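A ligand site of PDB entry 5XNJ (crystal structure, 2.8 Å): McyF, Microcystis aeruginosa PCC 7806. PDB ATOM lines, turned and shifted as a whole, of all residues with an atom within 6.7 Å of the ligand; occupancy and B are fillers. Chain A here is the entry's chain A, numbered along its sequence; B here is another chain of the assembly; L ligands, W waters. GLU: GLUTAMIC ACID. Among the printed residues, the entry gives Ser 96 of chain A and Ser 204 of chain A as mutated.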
ATOM      1  N   GLY A  22       0.242 -26.847  32.533  1.00  0.00           N
ATOM      2  CA  GLY A  22       1.015 -26.452  31.377  1.00  0.00           C
ATOM      3  C   GLY A  22       0.141 -26.074  30.203  1.00  0.00           C
ATOM      4  O   GLY A  22       0.647 -25.746  29.144  1.00  0.00           O
ATOM      5  N   MET A  23      -1.178 -26.104  30.386  1.00  0.00           N
ATOM      6  CA  MET A  23      -2.118 -25.850  29.300  1.00  0.00           C
ATOM      7  C   MET A  23      -2.641 -24.454  29.592  1.00  0.00           C
ATOM      8  O   MET A  23      -3.802 -24.211  29.905  1.00  0.00           O
ATOM      9  CB  MET A  23      -3.141 -26.941  29.230  1.00  0.00           C
ATOM     10  CG  MET A  23      -2.450 -28.228  28.786  1.00  0.00           C
ATOM     11  SD  MET A  23      -3.436 -29.714  28.824  1.00  0.00           S
ATOM     12  CE  MET A  23      -3.728 -29.835  30.590  1.00  0.00           C
ATOM     13  N   GLY A  24      -1.575 -23.703  29.701  1.00  0.00           N
ATOM     14  CA  GLY A  24      -1.473 -22.340  30.069  1.00  0.00           C
ATOM     15  C   GLY A  24      -0.407 -22.478  31.129  1.00  0.00           C
ATOM     16  O   GLY A  24      -0.714 -22.687  32.263  1.00  0.00           O
ATOM     17  N   VAL A  27      -0.832 -19.488  33.588  1.00  0.00           N
ATOM     18  CA  VAL A  27      -1.961 -19.688  34.504  1.00  0.00           C
ATOM     19  C   VAL A  27      -1.765 -20.877  35.450  1.00  0.00           C
ATOM     20  O   VAL A  27      -2.220 -20.821  36.587  1.00  0.00           O
ATOM     21  CB  VAL A  27      -3.327 -19.783  33.753  1.00  0.00           C
ATOM     22  CG1 VAL A  27      -3.462 -21.074  32.942  1.00  0.00           C
ATOM     23  CG2 VAL A  27      -4.481 -19.647  34.728  1.00  0.00           C
ATOM     24  N   ASP A  61      -1.651 -28.199  21.348  1.00  0.00           N
ATOM     25  CA  ASP A  61      -2.721 -27.189  21.477  1.00  0.00           C
ATOM     26  C   ASP A  61      -4.098 -27.861  21.461  1.00  0.00           C
ATOM     27  O   ASP A  61      -4.344 -28.772  20.671  1.00  0.00           O
ATOM     28  CB  ASP A  61      -2.655 -26.132  20.364  1.00  0.00           C
ATOM     29  CG  ASP A  61      -3.648 -24.999  20.589  1.00  0.00           C
ATOM     30  OD1 ASP A  61      -3.951 -24.654  21.754  1.00  0.00           O
ATOM     31  OD2 ASP A  61      -4.163 -24.438  19.586  1.00  0.00           O
ATOM     32  N   ARG A  62      -4.963 -27.415  22.364  1.00  0.00           N
ATOM     33  CA  ARG A  62      -6.238 -28.099  22.619  1.00  0.00           C
ATOM     34  C   ARG A  62      -7.210 -27.844  21.462  1.00  0.00           C
ATOM     35  O   ARG A  62      -7.709 -28.785  20.848  1.00  0.00           O
ATOM     36  CB  ARG A  62      -6.840 -27.658  23.962  1.00  0.00           C
ATOM     37  CG  ARG A  62      -6.315 -28.411  25.183  1.00  0.00           C
ATOM     38  CD  ARG A  62      -4.800 -28.388  25.351  1.00  0.00           C
ATOM     39  NE  ARG A  62      -4.248 -27.063  25.676  1.00  0.00           N
ATOM     40  CZ  ARG A  62      -2.956 -26.719  25.603  1.00  0.00           C
ATOM     41  NH1 ARG A  62      -2.581 -25.495  25.943  1.00  0.00           N
ATOM     42  NH2 ARG A  62      -2.025 -27.588  25.210  1.00  0.00           N
ATOM     43  N   THR A  63      -7.436 -26.555  21.194  1.00  0.00           N
ATOM     44  CA  THR A  63      -8.264 -26.104  20.072  1.00  0.00           C
ATOM     45  C   THR A  63      -7.681 -26.578  18.727  1.00  0.00           C
ATOM     46  O   THR A  63      -8.407 -27.077  17.862  1.00  0.00           O
ATOM     47  CB  THR A  63      -8.409 -24.568  20.072  1.00  0.00           C
ATOM     48  OG1 THR A  63      -8.755 -24.117  21.394  1.00  0.00           O
ATOM     49  CG2 THR A  63      -9.463 -24.099  19.065  1.00  0.00           C
ATOM     50  N   GLY A  95      -5.759 -28.446  34.249  1.00  0.00           N
ATOM     51  CA  GLY A  95      -5.707 -26.977  34.225  1.00  0.00           C
ATOM     52  C   GLY A  95      -6.200 -26.279  32.970  1.00  0.00           C
ATOM     53  O   GLY A  95      -5.758 -25.162  32.649  1.00  0.00           O
ATOM     54  N   SER A  96      -7.139 -26.913  32.288  1.00  0.00           N
ATOM     55  CA  SER A  96      -7.661 -26.419  31.017  1.00  0.00           C
ATOM     56  C   SER A  96      -9.084 -26.936  30.862  1.00  0.00           C
ATOM     57  O   SER A  96      -9.313 -28.146  30.929  1.00  0.00           O
ATOM     58  CB  SER A  96      -6.786 -26.919  29.856  1.00  0.00           C
ATOM     59  OG  SER A  96      -7.498 -26.933  28.627  1.00  0.00           O
ATOM     60  N   CYS A  97     -10.026 -26.026  30.685  1.00  0.00           N
ATOM     61  CA  CYS A  97     -11.397 -26.418  30.379  1.00  0.00           C
ATOM     62  C   CYS A  97     -11.469 -27.180  29.053  1.00  0.00           C
ATOM     63  O   CYS A  97     -11.956 -28.312  29.016  1.00  0.00           O
ATOM     64  CB  CYS A  97     -12.302 -25.201  30.366  1.00  0.00           C
ATOM     65  SG  CYS A  97     -12.451 -24.452  32.007  1.00  0.00           S
ATOM     66  N   THR A  98     -10.974 -26.599  27.950  1.00  0.00           N
ATOM     67  CA  THR A  98     -11.019 -27.288  26.646  1.00  0.00           C
ATOM     68  C   THR A  98     -10.467 -28.719  26.688  1.00  0.00           C
ATOM     69  O   THR A  98     -10.960 -29.593  25.983  1.00  0.00           O
ATOM     70  CB  THR A  98     -10.281 -26.517  25.537  1.00  0.00           C
ATOM     71  OG1 THR A  98     -10.777 -25.179  25.467  1.00  0.00           O
ATOM     72  CG2 THR A  98     -10.485 -27.191  24.191  1.00  0.00           C
ATOM     73  N   ALA A  99      -9.433 -28.947  27.488  1.00  0.00           N
ATOM     74  CA  ALA A  99      -8.860 -30.289  27.606  1.00  0.00           C
ATOM     75  C   ALA A  99      -9.812 -31.337  28.178  1.00  0.00           C
ATOM     76  O   ALA A  99      -9.577 -32.530  28.004  1.00  0.00           O
ATOM     77  CB  ALA A  99      -7.589 -30.259  28.426  1.00  0.00           C
ATOM     78  N   HIS A 100     -10.871 -30.901  28.863  1.00  0.00           N
ATOM     79  CA  HIS A 100     -11.900 -31.834  29.367  1.00  0.00           C
ATOM     80  C   HIS A 100     -12.660 -32.564  28.248  1.00  0.00           C
ATOM     81  O   HIS A 100     -13.308 -33.571  28.514  1.00  0.00           O
ATOM     82  CB  HIS A 100     -12.891 -31.121  30.295  1.00  0.00           C
ATOM     83  CG  HIS A 100     -12.316 -30.736  31.621  1.00  0.00           C
ATOM     84  ND1 HIS A 100     -11.363 -29.738  31.781  1.00  0.00           N
ATOM     85  CD2 HIS A 100     -12.566 -31.206  32.866  1.00  0.00           C
ATOM     86  CE1 HIS A 100     -11.055 -29.622  33.060  1.00  0.00           C
ATOM     87  NE2 HIS A 100     -11.760 -30.507  33.737  1.00  0.00           N
ATOM     88  N   LEU A 117     -13.514 -29.073  36.262  1.00  0.00           N
ATOM     89  CA  LEU A 117     -13.715 -27.641  36.189  1.00  0.00           C
ATOM     90  C   LEU A 117     -15.117 -27.250  35.698  1.00  0.00           C
ATOM     91  O   LEU A 117     -15.641 -26.202  36.074  1.00  0.00           O
ATOM     92  CB  LEU A 117     -12.667 -27.006  35.271  1.00  0.00           C
ATOM     93  CG  LEU A 117     -11.197 -27.132  35.668  1.00  0.00           C
ATOM     94  CD1 LEU A 117     -10.378 -26.270  34.720  1.00  0.00           C
ATOM     95  CD2 LEU A 117     -10.929 -26.728  37.116  1.00  0.00           C
ATOM     96  N   ALA A 136     -14.848 -18.371  26.639  1.00  0.00           N
ATOM     97  CA  ALA A 136     -14.041 -19.576  26.394  1.00  0.00           C
ATOM     98  C   ALA A 136     -13.447 -19.593  25.016  1.00  0.00           C
ATOM     99  O   ALA A 136     -13.786 -18.758  24.174  1.00  0.00           O
ATOM    100  CB  ALA A 136     -14.867 -20.832  26.614  1.00  0.00           C
ATOM    101  N   SER A 137     -12.550 -20.556  24.797  1.00  0.00           N
ATOM    102  CA  SER A 137     -11.992 -20.852  23.471  1.00  0.00           C
ATOM    103  C   SER A 137     -13.050 -21.363  22.488  1.00  0.00           C
ATOM    104  O   SER A 137     -14.021 -22.021  22.894  1.00  0.00           O
ATOM    105  CB  SER A 137     -10.870 -21.910  23.585  1.00  0.00           C
ATOM    106  OG  SER A 137     -11.354 -23.167  23.993  1.00  0.00           O
ATOM    107  N   THR A 140     -13.637 -25.007  23.006  1.00  0.00           N
ATOM    108  CA  THR A 140     -14.531 -25.243  24.132  1.00  0.00           C
ATOM    109  C   THR A 140     -15.969 -25.010  23.695  1.00  0.00           C
ATOM    110  O   THR A 140     -16.855 -25.749  24.100  1.00  0.00           O
ATOM    111  CB  THR A 140     -14.134 -24.335  25.319  1.00  0.00           C
ATOM    112  OG1 THR A 140     -12.916 -24.842  25.886  1.00  0.00           O
ATOM    113  CG2 THR A 140     -15.190 -24.305  26.407  1.00  0.00           C
ATOM    114  N   HIS A 168     -10.937 -15.687  21.942  1.00  0.00           N
ATOM    115  CA  HIS A 168      -9.818 -16.545  21.551  1.00  0.00           C
ATOM    116  C   HIS A 168      -8.535 -15.733  21.370  1.00  0.00           C
ATOM    117  O   HIS A 168      -7.464 -16.178  21.795  1.00  0.00           O
ATOM    118  CB  HIS A 168     -10.144 -17.298  20.260  1.00  0.00           C
ATOM    119  CG  HIS A 168      -9.290 -18.508  20.037  1.00  0.00           C
ATOM    120  ND1 HIS A 168      -9.591 -19.743  20.592  1.00  0.00           N
ATOM    121  CD2 HIS A 168      -8.179 -18.692  19.293  1.00  0.00           C
ATOM    122  CE1 HIS A 168      -8.686 -20.626  20.207  1.00  0.00           C
ATOM    123  NE2 HIS A 168      -7.814 -20.019  19.424  1.00  0.00           N
ATOM    124  N   ILE A 171      -7.140 -14.674  24.788  1.00  0.00           N
ATOM    125  CA  ILE A 171      -6.515 -15.769  25.483  1.00  0.00           C
ATOM    126  C   ILE A 171      -5.087 -15.992  24.989  1.00  0.00           C
ATOM    127  O   ILE A 171      -4.155 -16.080  25.789  1.00  0.00           O
ATOM    128  CB  ILE A 171      -7.337 -17.078  25.386  1.00  0.00           C
ATOM    129  CG1 ILE A 171      -8.699 -16.909  26.074  1.00  0.00           C
ATOM    130  CG2 ILE A 171      -6.572 -18.227  26.054  1.00  0.00           C
ATOM    131  CD1 ILE A 171      -9.774 -17.883  25.590  1.00  0.00           C
ATOM    132  N   TYR A 172      -4.910 -16.070  23.670  1.00  0.00           N
ATOM    133  CA  TYR A 172      -3.634 -16.425  23.077  1.00  0.00           C
ATOM    134  C   TYR A 172      -2.673 -15.239  22.937  1.00  0.00           C
ATOM    135  O   TYR A 172      -1.479 -15.388  23.198  1.00  0.00           O
ATOM    136  CB  TYR A 172      -3.832 -17.119  21.720  1.00  0.00           C
ATOM    137  CG  TYR A 172      -4.193 -18.589  21.851  1.00  0.00           C
ATOM    138  CD1 TYR A 172      -5.478 -18.988  22.212  1.00  0.00           C
ATOM    139  CD2 TYR A 172      -3.242 -19.596  21.620  1.00  0.00           C
ATOM    140  CE1 TYR A 172      -5.805 -20.333  22.340  1.00  0.00           C
ATOM    141  CE2 TYR A 172      -3.564 -20.940  21.739  1.00  0.00           C
ATOM    142  CZ  TYR A 172      -4.852 -21.309  22.101  1.00  0.00           C
ATOM    143  OH  TYR A 172      -5.206 -22.648  22.239  1.00  0.00           O
ATOM    144  N   LYS A 176      -2.131 -15.779  27.640  1.00  0.00           N
ATOM    145  CA  LYS A 176      -1.122 -16.851  27.598  1.00  0.00           C
ATOM    146  C   LYS A 176       0.326 -16.328  27.520  1.00  0.00           C
ATOM    147  O   LYS A 176       1.243 -17.003  27.957  1.00  0.00           O
ATOM    148  CB  LYS A 176      -1.367 -17.823  26.433  1.00  0.00           C
ATOM    149  CG  LYS A 176      -2.456 -18.830  26.709  1.00  0.00           C
ATOM    150  CD  LYS A 176      -2.727 -19.670  25.480  1.00  0.00           C
ATOM    151  CE  LYS A 176      -3.809 -20.696  25.746  1.00  0.00           C
ATOM    152  NZ  LYS A 176      -3.344 -21.884  26.509  1.00  0.00           N
ATOM    153  N   SER A 202     -15.339 -18.317  33.755  1.00  0.00           N
ATOM    154  CA  SER A 202     -14.022 -18.639  33.185  1.00  0.00           C
ATOM    155  C   SER A 202     -14.118 -19.959  32.434  1.00  0.00           C
ATOM    156  O   SER A 202     -13.745 -21.024  32.955  1.00  0.00           O
ATOM    157  CB  SER A 202     -12.946 -18.707  34.280  1.00  0.00           C
ATOM    158  OG  SER A 202     -12.674 -17.414  34.790  1.00  0.00           O
ATOM    159  N   GLY A 203     -14.622 -19.898  31.203  1.00  0.00           N
ATOM    160  CA  GLY A 203     -14.671 -21.076  30.334  1.00  0.00           C
ATOM    161  C   GLY A 203     -13.309 -21.443  29.770  1.00  0.00           C
ATOM    162  O   GLY A 203     -13.095 -22.575  29.357  1.00  0.00           O
ATOM    163  N   SER A 204     -12.422 -20.462  29.727  1.00  0.00           N
ATOM    164  CA  SER A 204     -10.991 -20.661  29.561  1.00  0.00           C
ATOM    165  C   SER A 204     -10.357 -20.433  30.932  1.00  0.00           C
ATOM    166  O   SER A 204     -10.672 -19.427  31.595  1.00  0.00           O
ATOM    167  CB  SER A 204     -10.411 -19.681  28.533  1.00  0.00           C
ATOM    168  OG  SER A 204      -9.006 -19.565  28.612  1.00  0.00           O
ATOM    169  N   THR A 205      -9.480 -21.354  31.356  1.00  0.00           N
ATOM    170  CA  THR A 205      -8.708 -21.193  32.597  1.00  0.00           C
ATOM    171  C   THR A 205      -7.893 -19.901  32.621  1.00  0.00           C
ATOM    172  O   THR A 205      -7.734 -19.317  33.690  1.00  0.00           O
ATOM    173  CB  THR A 205      -7.795 -22.387  32.929  1.00  0.00           C
ATOM    174  OG1 THR A 205      -7.053 -22.782  31.771  1.00  0.00           O
ATOM    175  CG2 THR A 205      -8.597 -23.573  33.403  1.00  0.00           C
ATOM    176  N   GLU A 206      -7.423 -19.421  31.473  1.00  0.00           N
ATOM    177  CA  GLU A 206      -6.643 -18.182  31.464  1.00  0.00           C
ATOM    178  C   GLU A 206      -7.389 -16.990  32.061  1.00  0.00           C
ATOM    179  O   GLU A 206      -6.736 -15.997  32.420  1.00  0.00           O
ATOM    180  CB  GLU A 206      -6.100 -17.840  30.056  1.00  0.00           C
ATOM    181  CG  GLU A 206      -4.722 -18.441  29.752  1.00  0.00           C
ATOM    182  CD  GLU A 206      -4.766 -19.882  29.281  1.00  0.00           C
ATOM    183  OE1 GLU A 206      -3.711 -20.565  29.237  1.00  0.00           O
ATOM    184  OE2 GLU A 206      -5.863 -20.341  28.933  1.00  0.00           O
ATOM    185  N   GLU B  45       3.016 -21.813  22.911  1.00  0.00           N
ATOM    186  CA  GLU B  45       3.279 -22.351  24.263  1.00  0.00           C
ATOM    187  C   GLU B  45       4.072 -23.653  24.291  1.00  0.00           C
ATOM    188  O   GLU B  45       4.744 -23.933  25.267  1.00  0.00           O
ATOM    189  CB  GLU B  45       1.990 -22.700  24.984  1.00  0.00           C
ATOM    190  CG  GLU B  45       1.071 -21.542  25.281  1.00  0.00           C
ATOM    191  CD  GLU B  45      -0.112 -21.985  26.100  1.00  0.00           C
ATOM    192  OE1 GLU B  45      -0.753 -22.998  25.766  1.00  0.00           O
ATOM    193  OE2 GLU B  45      -0.404 -21.275  27.064  1.00  0.00           O
HETATM  194  N   GLU L   1      -6.606 -22.660  28.852  1.00  0.00           N
HETATM  195  CA  GLU L   1      -7.975 -22.521  28.248  1.00  0.00           C
HETATM  196  C   GLU L   1      -8.834 -23.643  28.713  1.00  0.00           C
HETATM  197  O   GLU L   1      -9.413 -23.567  29.780  1.00  0.00           O
HETATM  198  CB  GLU L   1      -8.002 -22.398  26.696  1.00  0.00           C
HETATM  199  CG  GLU L   1      -6.829 -22.933  25.866  1.00  0.00           C
HETATM  200  CD  GLU L   1      -6.117 -24.163  26.432  1.00  0.00           C
HETATM  201  OE1 GLU L   1      -6.773 -25.093  26.926  1.00  0.00           O
HETATM  202  OE2 GLU L   1      -4.868 -24.180  26.399  1.00  0.00           O
HETATM  203  OXT GLU L   1      -8.949 -24.669  28.063  1.00  0.00           O
HETATM  204  O   HOH W   1      -8.174 -20.424  24.364  1.00  0.00           O
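Merely in contact with the ligand: Ser 204 (3.2 Å), Gly 203 (3.8 Å) and Tyr 172 (3.98 Å).
An oxygen (OE2) of the ligand lies within salt-bridge range of the side-chain amino group of Lys 176 (2.8 Å).
An oxygen (OE2) of the ligand lies within salt-bridge range of the guanidinium group of Arg 62, 2.7 Å away.
N of the ligand is in hydrogen-bond range of OG1 of Thr 205, 3.0 Å away.
The backbone NH of Thr 205 sits at hydrogen-bond distance from an oxygen (O) of the ligand (2.7 Å).
The backbone NH (N) of Cys 97 is in hydrogen-bond range of an oxygen (O) of the ligand, at 2.7 Å.
OG1 of Thr 98 sits at hydrogen-bond distance from OXT of the ligand (3.2 Å).
N of the ligand is in hydrogen-bond range of O of Met 23, at 3.4 Å.
The backbone NH (N) of Thr 98 is in hydrogen-bond range of an oxygen (OXT) of the ligand.
The side-chain hydroxyl (OG) of Ser 96 lies within hydrogen-bond range of an oxygen (OE1) of the ligand.
N of the ligand lies within salt-bridge range of OE2 of Glu 206, 2.4 Å away.
OH of Tyr 172 lies within hydrogen-bond range of OD1 of Asp 61.
The side-chain hydroxyl of Thr 98 sits at hydrogen-bond distance from the side-chain hydroxyl of Ser 137, 2.6 Å away.
OG of Ser 204 lies within hydrogen-bond range of OE2 of Glu 206 (3.3 Å).
The side-chain hydroxyl of Thr 205 sits at hydrogen-bond distance from the backbone carbonyl oxygen of Gly 95.
O of Gly 203 lies close to SG of Cys 97, at 3.3 Å.
The backbone carbonyl oxygen (O) of Ser 202 lies within hydrogen-bond range of the side-chain sulfur (SG) of Cys 97, at 3.8 Å.
N of Ala 99 is in hydrogen-bond range of OG of Ser 96 (3.0 Å).
A ring nitrogen (ND1) of His 100 is in hydrogen-bond range of the backbone carbonyl oxygen (O) of Cys 97.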
